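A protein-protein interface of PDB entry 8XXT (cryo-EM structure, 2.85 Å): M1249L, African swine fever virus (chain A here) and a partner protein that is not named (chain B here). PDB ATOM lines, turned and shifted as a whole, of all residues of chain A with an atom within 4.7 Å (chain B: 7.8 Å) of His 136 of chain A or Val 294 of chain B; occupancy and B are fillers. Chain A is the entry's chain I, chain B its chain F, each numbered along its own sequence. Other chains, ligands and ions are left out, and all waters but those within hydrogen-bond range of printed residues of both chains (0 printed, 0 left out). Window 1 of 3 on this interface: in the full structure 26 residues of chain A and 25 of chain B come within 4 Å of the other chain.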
ATOM      1  N   PRO A  74       9.805  10.370   0.910  1.00  0.00           N
ATOM      2  CA  PRO A  74       8.696  10.577  -0.035  1.00  0.00           C
ATOM      3  C   PRO A  74       8.067   9.287  -0.526  1.00  0.00           C
ATOM      4  O   PRO A  74       6.858   9.265  -0.788  1.00  0.00           O
ATOM      5  CB  PRO A  74       9.354  11.360  -1.181  1.00  0.00           C
ATOM      6  CG  PRO A  74      10.828  11.170  -0.996  1.00  0.00           C
ATOM      7  CD  PRO A  74      11.023  11.070   0.476  1.00  0.00           C
ATOM      8  N   GLY A  78       4.135   8.744   0.011  1.00  0.00           N
ATOM      9  CA  GLY A  78       3.250   8.536  -1.121  1.00  0.00           C
ATOM     10  C   GLY A  78       2.497   7.225  -1.034  1.00  0.00           C
ATOM     11  O   GLY A  78       1.317   7.154  -1.382  1.00  0.00           O
ATOM     12  N   PHE A  89      -2.092   7.319  -6.731  1.00  0.00           N
ATOM     13  CA  PHE A  89      -0.987   6.942  -7.608  1.00  0.00           C
ATOM     14  C   PHE A  89      -0.858   5.429  -7.729  1.00  0.00           C
ATOM     15  O   PHE A  89      -0.709   4.896  -8.833  1.00  0.00           O
ATOM     16  CB  PHE A  89       0.313   7.550  -7.094  1.00  0.00           C
ATOM     17  CG  PHE A  89       0.358   9.037  -7.197  1.00  0.00           C
ATOM     18  CD1 PHE A  89       0.364   9.655  -8.431  1.00  0.00           C
ATOM     19  CD2 PHE A  89       0.381   9.821  -6.060  1.00  0.00           C
ATOM     20  CE1 PHE A  89       0.401  11.027  -8.529  1.00  0.00           C
ATOM     21  CE2 PHE A  89       0.419  11.194  -6.153  1.00  0.00           C
ATOM     22  CZ  PHE A  89       0.427  11.796  -7.390  1.00  0.00           C
ATOM     23  N   PHE A 130       8.764   6.268  -9.812  1.00  0.00           N
ATOM     24  CA  PHE A 130       8.113   7.568  -9.712  1.00  0.00           C
ATOM     25  C   PHE A 130       8.029   8.025  -8.262  1.00  0.00           C
ATOM     26  O   PHE A 130       8.200   9.214  -7.968  1.00  0.00           O
ATOM     27  CB  PHE A 130       6.722   7.504 -10.339  1.00  0.00           C
ATOM     28  CG  PHE A 130       5.874   8.710 -10.064  1.00  0.00           C
ATOM     29  CD1 PHE A 130       6.286   9.968 -10.466  1.00  0.00           C
ATOM     30  CD2 PHE A 130       4.659   8.583  -9.414  1.00  0.00           C
ATOM     31  CE1 PHE A 130       5.504  11.076 -10.218  1.00  0.00           C
ATOM     32  CE2 PHE A 130       3.873   9.689  -9.165  1.00  0.00           C
ATOM     33  CZ  PHE A 130       4.296  10.937  -9.568  1.00  0.00           C
ATOM     34  N   LEU A 131       7.766   7.094  -7.341  1.00  0.00           N
ATOM     35  CA  LEU A 131       7.695   7.449  -5.928  1.00  0.00           C
ATOM     36  C   LEU A 131       9.032   7.962  -5.415  1.00  0.00           C
ATOM     37  O   LEU A 131       9.069   8.883  -4.592  1.00  0.00           O
ATOM     38  CB  LEU A 131       7.227   6.248  -5.106  1.00  0.00           C
ATOM     39  CG  LEU A 131       5.803   5.764  -5.389  1.00  0.00           C
ATOM     40  CD1 LEU A 131       5.484   4.518  -4.584  1.00  0.00           C
ATOM     41  CD2 LEU A 131       4.791   6.858  -5.105  1.00  0.00           C
ATOM     42  N   SER A 133      11.051   9.385  -7.492  1.00  0.00           N
ATOM     43  CA  SER A 133      11.363  10.491  -8.386  1.00  0.00           C
ATOM     44  C   SER A 133      11.104  11.826  -7.704  1.00  0.00           C
ATOM     45  O   SER A 133      10.328  11.925  -6.749  1.00  0.00           O
ATOM     46  CB  SER A 133      10.540  10.394  -9.667  1.00  0.00           C
ATOM     47  OG  SER A 133       9.205  10.805  -9.436  1.00  0.00           O
ATOM     48  N   GLY A 134      11.769  12.864  -8.210  1.00  0.00           N
ATOM     49  CA  GLY A 134      11.676  14.169  -7.580  1.00  0.00           C
ATOM     50  C   GLY A 134      10.281  14.756  -7.629  1.00  0.00           C
ATOM     51  O   GLY A 134       9.838  15.403  -6.677  1.00  0.00           O
ATOM     52  N   GLY A 135       9.576  14.552  -8.741  1.00  0.00           N
ATOM     53  CA  GLY A 135       8.271  15.173  -8.901  1.00  0.00           C
ATOM     54  C   GLY A 135       7.265  14.702  -7.870  1.00  0.00           C
ATOM     55  O   GLY A 135       6.550  15.507  -7.265  1.00  0.00           O
ATOM     56  N   HIS A 136       7.195  13.387  -7.654  1.00  0.00           N
ATOM     57  CA  HIS A 136       6.290  12.879  -6.632  1.00  0.00           C
ATOM     58  C   HIS A 136       6.727  13.302  -5.239  1.00  0.00           C
ATOM     59  O   HIS A 136       5.880  13.518  -4.370  1.00  0.00           O
ATOM     60  CB  HIS A 136       6.191  11.360  -6.697  1.00  0.00           C
ATOM     61  CG  HIS A 136       5.450  10.767  -5.542  1.00  0.00           C
ATOM     62  ND1 HIS A 136       4.076  10.745  -5.473  1.00  0.00           N
ATOM     63  CD2 HIS A 136       5.895  10.194  -4.400  1.00  0.00           C
ATOM     64  CE1 HIS A 136       3.703  10.173  -4.342  1.00  0.00           C
ATOM     65  NE2 HIS A 136       4.789   9.831  -3.672  1.00  0.00           N
ATOM     66  N   SER A 137       8.037  13.418  -5.006  1.00  0.00           N
ATOM     67  CA  SER A 137       8.506  13.918  -3.719  1.00  0.00           C
ATOM     68  C   SER A 137       8.001  15.333  -3.471  1.00  0.00           C
ATOM     69  O   SER A 137       7.486  15.635  -2.390  1.00  0.00           O
ATOM     70  CB  SER A 137      10.030  13.879  -3.668  1.00  0.00           C
ATOM     71  OG  SER A 137      10.586  14.800  -4.587  1.00  0.00           O
ATOM     72  N   TRP A 138       8.114  16.202  -4.478  1.00  0.00           N
ATOM     73  CA  TRP A 138       7.606  17.565  -4.349  1.00  0.00           C
ATOM     74  C   TRP A 138       6.099  17.574  -4.134  1.00  0.00           C
ATOM     75  O   TRP A 138       5.587  18.331  -3.300  1.00  0.00           O
ATOM     76  CB  TRP A 138       7.973  18.374  -5.592  1.00  0.00           C
ATOM     77  CG  TRP A 138       7.382  19.754  -5.652  1.00  0.00           C
ATOM     78  CD1 TRP A 138       7.980  20.917  -5.267  1.00  0.00           C
ATOM     79  CD2 TRP A 138       6.083  20.115  -6.141  1.00  0.00           C
ATOM     80  NE1 TRP A 138       7.133  21.977  -5.478  1.00  0.00           N
ATOM     81  CE2 TRP A 138       5.962  21.512  -6.013  1.00  0.00           C
ATOM     82  CE3 TRP A 138       5.011  19.394  -6.671  1.00  0.00           C
ATOM     83  CZ2 TRP A 138       4.814  22.198  -6.393  1.00  0.00           C
ATOM     84  CZ3 TRP A 138       3.870  20.076  -7.044  1.00  0.00           C
ATOM     85  CH2 TRP A 138       3.780  21.463  -6.905  1.00  0.00           C
ATOM     86  N   LEU A 139       5.371  16.744  -4.883  1.00  0.00           N
ATOM     87  CA  LEU A 139       3.917  16.741  -4.761  1.00  0.00           C
ATOM     88  C   LEU A 139       3.481  16.256  -3.384  1.00  0.00           C
ATOM     89  O   LEU A 139       2.571  16.832  -2.776  1.00  0.00           O
ATOM     90  CB  LEU A 139       3.309  15.898  -5.886  1.00  0.00           C
ATOM     91  CG  LEU A 139       1.820  15.552  -5.997  1.00  0.00           C
ATOM     92  CD1 LEU A 139       1.582  15.010  -7.386  1.00  0.00           C
ATOM     93  CD2 LEU A 139       1.348  14.523  -4.980  1.00  0.00           C
ATOM     94  N   ILE A 140       4.121  15.205  -2.869  1.00  0.00           N
ATOM     95  CA  ILE A 140       3.753  14.701  -1.552  1.00  0.00           C
ATOM     96  C   ILE A 140       4.176  15.676  -0.464  1.00  0.00           C
ATOM     97  O   ILE A 140       3.508  15.777   0.571  1.00  0.00           O
ATOM     98  CB  ILE A 140       4.332  13.290  -1.327  1.00  0.00           C
ATOM     99  CG1 ILE A 140       3.420  12.495  -0.395  1.00  0.00           C
ATOM    100  CG2 ILE A 140       5.748  13.345  -0.774  1.00  0.00           C
ATOM    101  CD1 ILE A 140       2.113  12.090  -1.030  1.00  0.00           C
ATOM    102  N   ASN B  82      16.791  14.870  -5.002  1.00  0.00           N
ATOM    103  CA  ASN B  82      16.124  13.637  -5.386  1.00  0.00           C
ATOM    104  C   ASN B  82      16.991  12.834  -6.349  1.00  0.00           C
ATOM    105  O   ASN B  82      18.101  13.230  -6.712  1.00  0.00           O
ATOM    106  CB  ASN B  82      14.770  13.948  -6.016  1.00  0.00           C
ATOM    107  CG  ASN B  82      14.003  15.001  -5.251  1.00  0.00           C
ATOM    108  OD1 ASN B  82      13.429  14.722  -4.201  1.00  0.00           O
ATOM    109  ND2 ASN B  82      13.994  16.220  -5.771  1.00  0.00           N
ATOM    110  N   TYR B 164       4.976   8.185 -22.330  1.00  0.00           N
ATOM    111  CA  TYR B 164       4.001   8.206 -21.250  1.00  0.00           C
ATOM    112  C   TYR B 164       2.609   8.075 -21.846  1.00  0.00           C
ATOM    113  O   TYR B 164       2.197   8.921 -22.644  1.00  0.00           O
ATOM    114  CB  TYR B 164       4.120   9.508 -20.454  1.00  0.00           C
ATOM    115  CG  TYR B 164       5.299   9.567 -19.509  1.00  0.00           C
ATOM    116  CD1 TYR B 164       5.905   8.409 -19.044  1.00  0.00           C
ATOM    117  CD2 TYR B 164       5.810  10.786 -19.089  1.00  0.00           C
ATOM    118  CE1 TYR B 164       6.985   8.467 -18.186  1.00  0.00           C
ATOM    119  CE2 TYR B 164       6.888  10.852 -18.231  1.00  0.00           C
ATOM    120  CZ  TYR B 164       7.471   9.689 -17.782  1.00  0.00           C
ATOM    121  OH  TYR B 164       8.545   9.749 -16.926  1.00  0.00           O
ATOM    122  N   LEU B 170      -7.039  15.347 -15.853  1.00  0.00           N
ATOM    123  CA  LEU B 170      -6.669  16.209 -14.741  1.00  0.00           C
ATOM    124  C   LEU B 170      -7.911  16.785 -14.075  1.00  0.00           C
ATOM    125  O   LEU B 170      -8.922  17.046 -14.733  1.00  0.00           O
ATOM    126  CB  LEU B 170      -5.778  17.347 -15.233  1.00  0.00           C
ATOM    127  CG  LEU B 170      -4.418  16.960 -15.812  1.00  0.00           C
ATOM    128  CD1 LEU B 170      -3.862  18.101 -16.632  1.00  0.00           C
ATOM    129  CD2 LEU B 170      -3.454  16.586 -14.706  1.00  0.00           C
ATOM    130  N   GLN B 174      -5.458  19.187  -9.166  1.00  0.00           N
ATOM    131  CA  GLN B 174      -4.208  18.855  -9.838  1.00  0.00           C
ATOM    132  C   GLN B 174      -3.800  19.966 -10.795  1.00  0.00           C
ATOM    133  O   GLN B 174      -2.609  20.270 -10.940  1.00  0.00           O
ATOM    134  CB  GLN B 174      -4.351  17.519 -10.568  1.00  0.00           C
ATOM    135  CG  GLN B 174      -4.997  16.433  -9.714  1.00  0.00           C
ATOM    136  CD  GLN B 174      -5.482  15.243 -10.524  1.00  0.00           C
ATOM    137  OE1 GLN B 174      -6.507  15.314 -11.201  1.00  0.00           O
ATOM    138  NE2 GLN B 174      -4.757  14.136 -10.442  1.00  0.00           N
ATOM    139  N   ASN B 177      -2.051  22.422  -8.725  1.00  0.00           N
ATOM    140  CA  ASN B 177      -0.711  21.955  -8.375  1.00  0.00           C
ATOM    141  C   ASN B 177       0.270  22.212  -9.514  1.00  0.00           C
ATOM    142  O   ASN B 177       1.330  22.831  -9.324  1.00  0.00           O
ATOM    143  CB  ASN B 177      -0.751  20.470  -8.019  1.00  0.00           C
ATOM    144  CG  ASN B 177      -1.689  20.174  -6.869  1.00  0.00           C
ATOM    145  OD1 ASN B 177      -2.344  21.072  -6.341  1.00  0.00           O
ATOM    146  ND2 ASN B 177      -1.761  18.909  -6.476  1.00  0.00           N
ATOM    147  N   LEU B 178      -0.080  21.771 -10.722  1.00  0.00           N
ATOM    148  CA  LEU B 178       0.814  22.045 -11.839  1.00  0.00           C
ATOM    149  C   LEU B 178       0.830  23.516 -12.237  1.00  0.00           C
ATOM    150  O   LEU B 178       1.782  23.939 -12.895  1.00  0.00           O
ATOM    151  CB  LEU B 178       0.496  21.167 -13.054  1.00  0.00           C
ATOM    152  CG  LEU B 178       0.667  19.642 -12.944  1.00  0.00           C
ATOM    153  CD1 LEU B 178       1.890  19.308 -12.103  1.00  0.00           C
ATOM    154  CD2 LEU B 178      -0.549  18.880 -12.468  1.00  0.00           C
ATOM    155  N   LEU B 181       3.556  24.669 -10.217  1.00  0.00           N
ATOM    156  CA  LEU B 181       4.782  24.199 -10.859  1.00  0.00           C
ATOM    157  C   LEU B 181       5.170  25.075 -12.052  1.00  0.00           C
ATOM    158  O   LEU B 181       6.353  25.401 -12.238  1.00  0.00           O
ATOM    159  CB  LEU B 181       4.621  22.740 -11.283  1.00  0.00           C
ATOM    160  CG  LEU B 181       5.490  21.749 -10.508  1.00  0.00           C
ATOM    161  CD1 LEU B 181       5.450  20.375 -11.148  1.00  0.00           C
ATOM    162  CD2 LEU B 181       6.916  22.258 -10.424  1.00  0.00           C
ATOM    163  N   VAL B 239       4.098  22.478 -23.275  1.00  0.00           N
ATOM    164  CA  VAL B 239       3.501  21.923 -22.064  1.00  0.00           C
ATOM    165  C   VAL B 239       2.959  23.038 -21.183  1.00  0.00           C
ATOM    166  O   VAL B 239       1.923  22.880 -20.527  1.00  0.00           O
ATOM    167  CB  VAL B 239       4.520  21.049 -21.311  1.00  0.00           C
ATOM    168  CG1 VAL B 239       3.856  20.362 -20.129  1.00  0.00           C
ATOM    169  CG2 VAL B 239       5.110  20.023 -22.247  1.00  0.00           C
ATOM    170  N   LEU B 243      -0.858  23.586 -20.224  1.00  0.00           N
ATOM    171  CA  LEU B 243      -1.257  23.753 -18.833  1.00  0.00           C
ATOM    172  C   LEU B 243      -2.262  24.886 -18.673  1.00  0.00           C
ATOM    173  O   LEU B 243      -3.324  24.698 -18.065  1.00  0.00           O
ATOM    174  CB  LEU B 243      -0.028  23.997 -17.961  1.00  0.00           C
ATOM    175  CG  LEU B 243       0.659  22.747 -17.419  1.00  0.00           C
ATOM    176  CD1 LEU B 243       1.956  23.128 -16.734  1.00  0.00           C
ATOM    177  CD2 LEU B 243      -0.268  21.999 -16.476  1.00  0.00           C
ATOM    178  N   SER B 288      -1.896   8.393 -14.826  1.00  0.00           N
ATOM    179  CA  SER B 288      -2.713   9.592 -14.957  1.00  0.00           C
ATOM    180  C   SER B 288      -1.892  10.788 -15.424  1.00  0.00           C
ATOM    181  O   SER B 288      -0.672  10.836 -15.270  1.00  0.00           O
ATOM    182  CB  SER B 288      -3.371   9.940 -13.624  1.00  0.00           C
ATOM    183  OG  SER B 288      -2.453  10.607 -12.775  1.00  0.00           O
ATOM    184  N   ALA B 289      -2.596  11.790 -15.961  1.00  0.00           N
ATOM    185  CA  ALA B 289      -1.930  12.965 -16.511  1.00  0.00           C
ATOM    186  C   ALA B 289      -1.269  13.819 -15.444  1.00  0.00           C
ATOM    187  O   ALA B 289      -0.372  14.602 -15.770  1.00  0.00           O
ATOM    188  CB  ALA B 289      -2.920  13.818 -17.301  1.00  0.00           C
ATOM    189  N   GLU B 290      -1.702  13.711 -14.187  1.00  0.00           N
ATOM    190  CA  GLU B 290      -1.003  14.401 -13.111  1.00  0.00           C
ATOM    191  C   GLU B 290       0.431  13.902 -12.998  1.00  0.00           C
ATOM    192  O   GLU B 290       1.368  14.694 -12.851  1.00  0.00           O
ATOM    193  CB  GLU B 290      -1.750  14.210 -11.794  1.00  0.00           C
ATOM    194  CG  GLU B 290      -1.062  14.826 -10.594  1.00  0.00           C
ATOM    195  CD  GLU B 290      -1.960  14.865  -9.378  1.00  0.00           C
ATOM    196  OE1 GLU B 290      -2.728  13.901  -9.180  1.00  0.00           O
ATOM    197  OE2 GLU B 290      -1.902  15.857  -8.621  1.00  0.00           O
ATOM    198  N   VAL B 291       0.617  12.583 -13.080  1.00  0.00           N
ATOM    199  CA  VAL B 291       1.957  12.004 -13.058  1.00  0.00           C
ATOM    200  C   VAL B 291       2.778  12.525 -14.223  1.00  0.00           C
ATOM    201  O   VAL B 291       3.923  12.955 -14.053  1.00  0.00           O
ATOM    202  CB  VAL B 291       1.868  10.468 -13.086  1.00  0.00           C
ATOM    203  CG1 VAL B 291       3.255   9.851 -13.040  1.00  0.00           C
ATOM    204  CG2 VAL B 291       1.005   9.965 -11.950  1.00  0.00           C
ATOM    205  N   MET B 292       2.205  12.500 -15.428  1.00  0.00           N
ATOM    206  CA  MET B 292       2.938  12.967 -16.597  1.00  0.00           C
ATOM    207  C   MET B 292       3.360  14.416 -16.443  1.00  0.00           C
ATOM    208  O   MET B 292       4.535  14.749 -16.629  1.00  0.00           O
ATOM    209  CB  MET B 292       2.096  12.798 -17.858  1.00  0.00           C
ATOM    210  CG  MET B 292       1.960  11.380 -18.363  1.00  0.00           C
ATOM    211  SD  MET B 292       1.468  10.133 -17.164  1.00  0.00           S
ATOM    212  CE  MET B 292       1.771   8.631 -18.091  1.00  0.00           C
ATOM    213  N   PHE B 293       2.416  15.301 -16.122  1.00  0.00           N
ATOM    214  CA  PHE B 293       2.771  16.711 -16.037  1.00  0.00           C
ATOM    215  C   PHE B 293       3.747  16.975 -14.903  1.00  0.00           C
ATOM    216  O   PHE B 293       4.676  17.766 -15.079  1.00  0.00           O
ATOM    217  CB  PHE B 293       1.525  17.583 -15.902  1.00  0.00           C
ATOM    218  CG  PHE B 293       0.865  17.888 -17.216  1.00  0.00           C
ATOM    219  CD1 PHE B 293       1.513  17.598 -18.405  1.00  0.00           C
ATOM    220  CD2 PHE B 293      -0.391  18.470 -17.269  1.00  0.00           C
ATOM    221  CE1 PHE B 293       0.924  17.876 -19.617  1.00  0.00           C
ATOM    222  CE2 PHE B 293      -0.984  18.749 -18.483  1.00  0.00           C
ATOM    223  CZ  PHE B 293      -0.325  18.450 -19.657  1.00  0.00           C
ATOM    224  N   VAL B 294       3.588  16.305 -13.761  1.00  0.00           N
ATOM    225  CA  VAL B 294       4.548  16.450 -12.670  1.00  0.00           C
ATOM    226  C   VAL B 294       5.947  16.073 -13.145  1.00  0.00           C
ATOM    227  O   VAL B 294       6.909  16.834 -12.971  1.00  0.00           O
ATOM    228  CB  VAL B 294       4.109  15.596 -11.465  1.00  0.00           C
ATOM    229  CG1 VAL B 294       5.297  15.216 -10.616  1.00  0.00           C
ATOM    230  CG2 VAL B 294       3.075  16.332 -10.627  1.00  0.00           C
ATOM    231  N   THR B 295       6.071  14.904 -13.781  1.00  0.00           N
ATOM    232  CA  THR B 295       7.383  14.417 -14.195  1.00  0.00           C
ATOM    233  C   THR B 295       8.019  15.338 -15.228  1.00  0.00           C
ATOM    234  O   THR B 295       9.169  15.761 -15.068  1.00  0.00           O
ATOM    235  CB  THR B 295       7.272  12.996 -14.748  1.00  0.00           C
ATOM    236  OG1 THR B 295       6.330  12.971 -15.827  1.00  0.00           O
ATOM    237  CG2 THR B 295       6.843  12.022 -13.663  1.00  0.00           C
ATOM    238  N   LEU B 296       7.286  15.664 -16.298  1.00  0.00           N
ATOM    239  CA  LEU B 296       7.861  16.515 -17.336  1.00  0.00           C
ATOM    240  C   LEU B 296       8.189  17.898 -16.794  1.00  0.00           C
ATOM    241  O   LEU B 296       9.258  18.450 -17.083  1.00  0.00           O
ATOM    242  CB  LEU B 296       6.929  16.619 -18.545  1.00  0.00           C
ATOM    243  CG  LEU B 296       6.207  15.374 -19.061  1.00  0.00           C
ATOM    244  CD1 LEU B 296       4.959  15.755 -19.849  1.00  0.00           C
ATOM    245  CD2 LEU B 296       7.147  14.534 -19.907  1.00  0.00           C
ATOM    246  N   LEU B 297       7.283  18.476 -15.998  1.00  0.00           N
ATOM    247  CA  LEU B 297       7.521  19.809 -15.467  1.00  0.00           C
ATOM    248  C   LEU B 297       8.768  19.841 -14.603  1.00  0.00           C
ATOM    249  O   LEU B 297       9.603  20.738 -14.753  1.00  0.00           O
ATOM    250  CB  LEU B 297       6.307  20.282 -14.672  1.00  0.00           C
ATOM    251  CG  LEU B 297       5.178  20.933 -15.466  1.00  0.00           C
ATOM    252  CD1 LEU B 297       3.911  20.943 -14.639  1.00  0.00           C
ATOM    253  CD2 LEU B 297       5.562  22.342 -15.887  1.00  0.00           C
ATOM    254  N   LYS B 298       8.939  18.861 -13.711  1.00  0.00           N
ATOM    255  CA  LYS B 298      10.135  18.902 -12.877  1.00  0.00           C
ATOM    256  C   LYS B 298      11.384  18.533 -13.661  1.00  0.00           C
ATOM    257  O   LYS B 298      12.483  18.975 -13.308  1.00  0.00           O
ATOM    258  CB  LYS B 298       9.997  18.005 -11.655  1.00  0.00           C
ATOM    259  CG  LYS B 298      10.893  18.493 -10.534  1.00  0.00           C
ATOM    260  CD  LYS B 298      10.926  17.552  -9.369  1.00  0.00           C
ATOM    261  CE  LYS B 298      10.152  18.141  -8.215  1.00  0.00           C
ATOM    262  NZ  LYS B 298      10.610  19.510  -7.866  1.00  0.00           N
ATOM    263  N   GLU B 299      11.248  17.740 -14.726  1.00  0.00           N
ATOM    264  CA  GLU B 299      12.384  17.538 -15.617  1.00  0.00           C
ATOM    265  C   GLU B 299      12.848  18.869 -16.185  1.00  0.00           C
ATOM    266  O   GLU B 299      14.040  19.196 -16.144  1.00  0.00           O
ATOM    267  CB  GLU B 299      12.015  16.565 -16.736  1.00  0.00           C
ATOM    268  CG  GLU B 299      12.233  15.109 -16.365  1.00  0.00           C
ATOM    269  CD  GLU B 299      11.196  14.186 -16.967  1.00  0.00           C
ATOM    270  OE1 GLU B 299      11.157  14.066 -18.209  1.00  0.00           O
ATOM    271  OE2 GLU B 299      10.423  13.577 -16.198  1.00  0.00           O
ATOM    272  N   ILE B 300      11.901  19.672 -16.671  1.00  0.00           N
ATOM    273  CA  ILE B 300      12.236  21.005 -17.165  1.00  0.00           C
ATOM    274  C   ILE B 300      12.845  21.844 -16.049  1.00  0.00           C
ATOM    275  O   ILE B 300      13.805  22.594 -16.272  1.00  0.00           O
ATOM    276  CB  ILE B 300      10.990  21.682 -17.765  1.00  0.00           C
ATOM    277  CG1 ILE B 300      10.321  20.770 -18.792  1.00  0.00           C
ATOM    278  CG2 ILE B 300      11.368  22.997 -18.416  1.00  0.00           C
ATOM    279  CD1 ILE B 300       8.848  21.053 -18.991  1.00  0.00           C
ATOM    280  N   ILE B 301      12.302  21.726 -14.831  1.00  0.00           N
ATOM    281  CA  ILE B 301      12.824  22.488 -13.696  1.00  0.00           C
ATOM    282  C   ILE B 301      14.303  22.195 -13.495  1.00  0.00           C
ATOM    283  O   ILE B 301      15.130  23.109 -13.405  1.00  0.00           O
ATOM    284  CB  ILE B 301      12.035  22.180 -12.408  1.00  0.00           C
ATOM    285  CG1 ILE B 301      10.544  22.498 -12.521  1.00  0.00           C
ATOM    286  CG2 ILE B 301      12.626  22.943 -11.234  1.00  0.00           C
ATOM    287  CD1 ILE B 301      10.207  23.655 -13.390  1.00  0.00           C
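Phe 89 of chain A touches Val 291 of chain B. Phe 130 of chain A touches Val 291 of chain B (CZ to CG1, 3.8 Å). Gly 134 of chain A touches Asn 82 of chain B. Lys 298 of chain B touches Gly 134 of chain A (CE to O, 3.2 Å). Val 294 of chain B touches Gly 135 of chain A. Gly 135 of chain A touches Lys 298 of chain B (N to CD, 3.3 Å). CG1 of Val 294 of chain B touches N of His 136 of chain A (3.96 Å). CB of Trp 138 of chain A touches CE of Lys 298 of chain B, 3.4 Å away. Glu 290 of chain B touches Leu 139 of chain A (OE2 to CD1, 3.8 Å). Leu 139 of chain A touches Val 294 of chain B (CD1 to CG2, 3.8 Å).
Val 294 of chain B touches just these residues of chain A: Gly 135 (3.4 Å), His 136 (3.96 Å) and Leu 139 (3.8 Å). Of chain B, only Val 294 and Lys 298 come within 4 Å of Gly 135 of chain A. Of the printed residues of chain B, Phe 130 of chain A touches Val 291 and Thr 295. Of the printed residues of chain A, Val 291 of chain B touches Phe 89 (3.6 Å) and Phe 130 (3.8 Å). Of the printed residues of chain A, Asn 177 of chain B touches Trp 138. Printed residues of chain A within 4 Å of Lys 298 of chain B: Gly 134 (3.2 Å), Gly 135 (3.3 Å) and Trp 138 (3.4 Å). Leu 170 of chain B touches none of the printed residues of chain A. Leu 297 of chain B touches none of the printed residues of chain A. The nearest residue of chain A that does not touch Val 294 of chain B is Phe 130 of chain A (4.2 Å). The nearest printed residue of chain A that does not touch Thr 295 of chain B is Ser 133 of chain A (5.0 Å).
The side-chain amide oxygen (OD1) of Asn 82 of chain B sits at hydrogen-bond distance from the side-chain hydroxyl (OG) of Ser 137 of chain A, at 2.9 Å.
Hydrophobic or aromatic side chains of chain A that line the printed part of chain B: Phe 89, Phe 130, Trp 138 and Leu 139. Printed residues of chain B that touch a printed residue of chain A: Asn 82, Asn 177, Leu 181, Glu 290, Val 291, Val 294, Thr 295 and Lys 298. Hydrophobic or aromatic side chains of chain B that line the printed part of chain A: Leu 181, Val 291 and Val 294. Along chain B the printed residues that touch a printed residue of chain A span positions 82 to 298.
The backbone carbonyl oxygen (O) of Val 291 of chain B sits at hydrogen-bond distance from the side-chain hydroxyl (OG1) of Thr 295 of chain B, 3.0 Å away. N of Glu 290 of chain B sits close to OG of Ser 288 of chain B, at 3.5 Å. The side-chain amide nitrogen (NE2) of Gln 174 of chain B sits at hydrogen-bond distance from the side-chain carboxylate (OE1) of Glu 290 of chain B (2.4 Å). The backbone carbonyl oxygen (O) of Met 292 of chain B is in hydrogen-bond range of the side-chain hydroxyl (OG1) of Thr 295 of chain B (2.7 Å).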
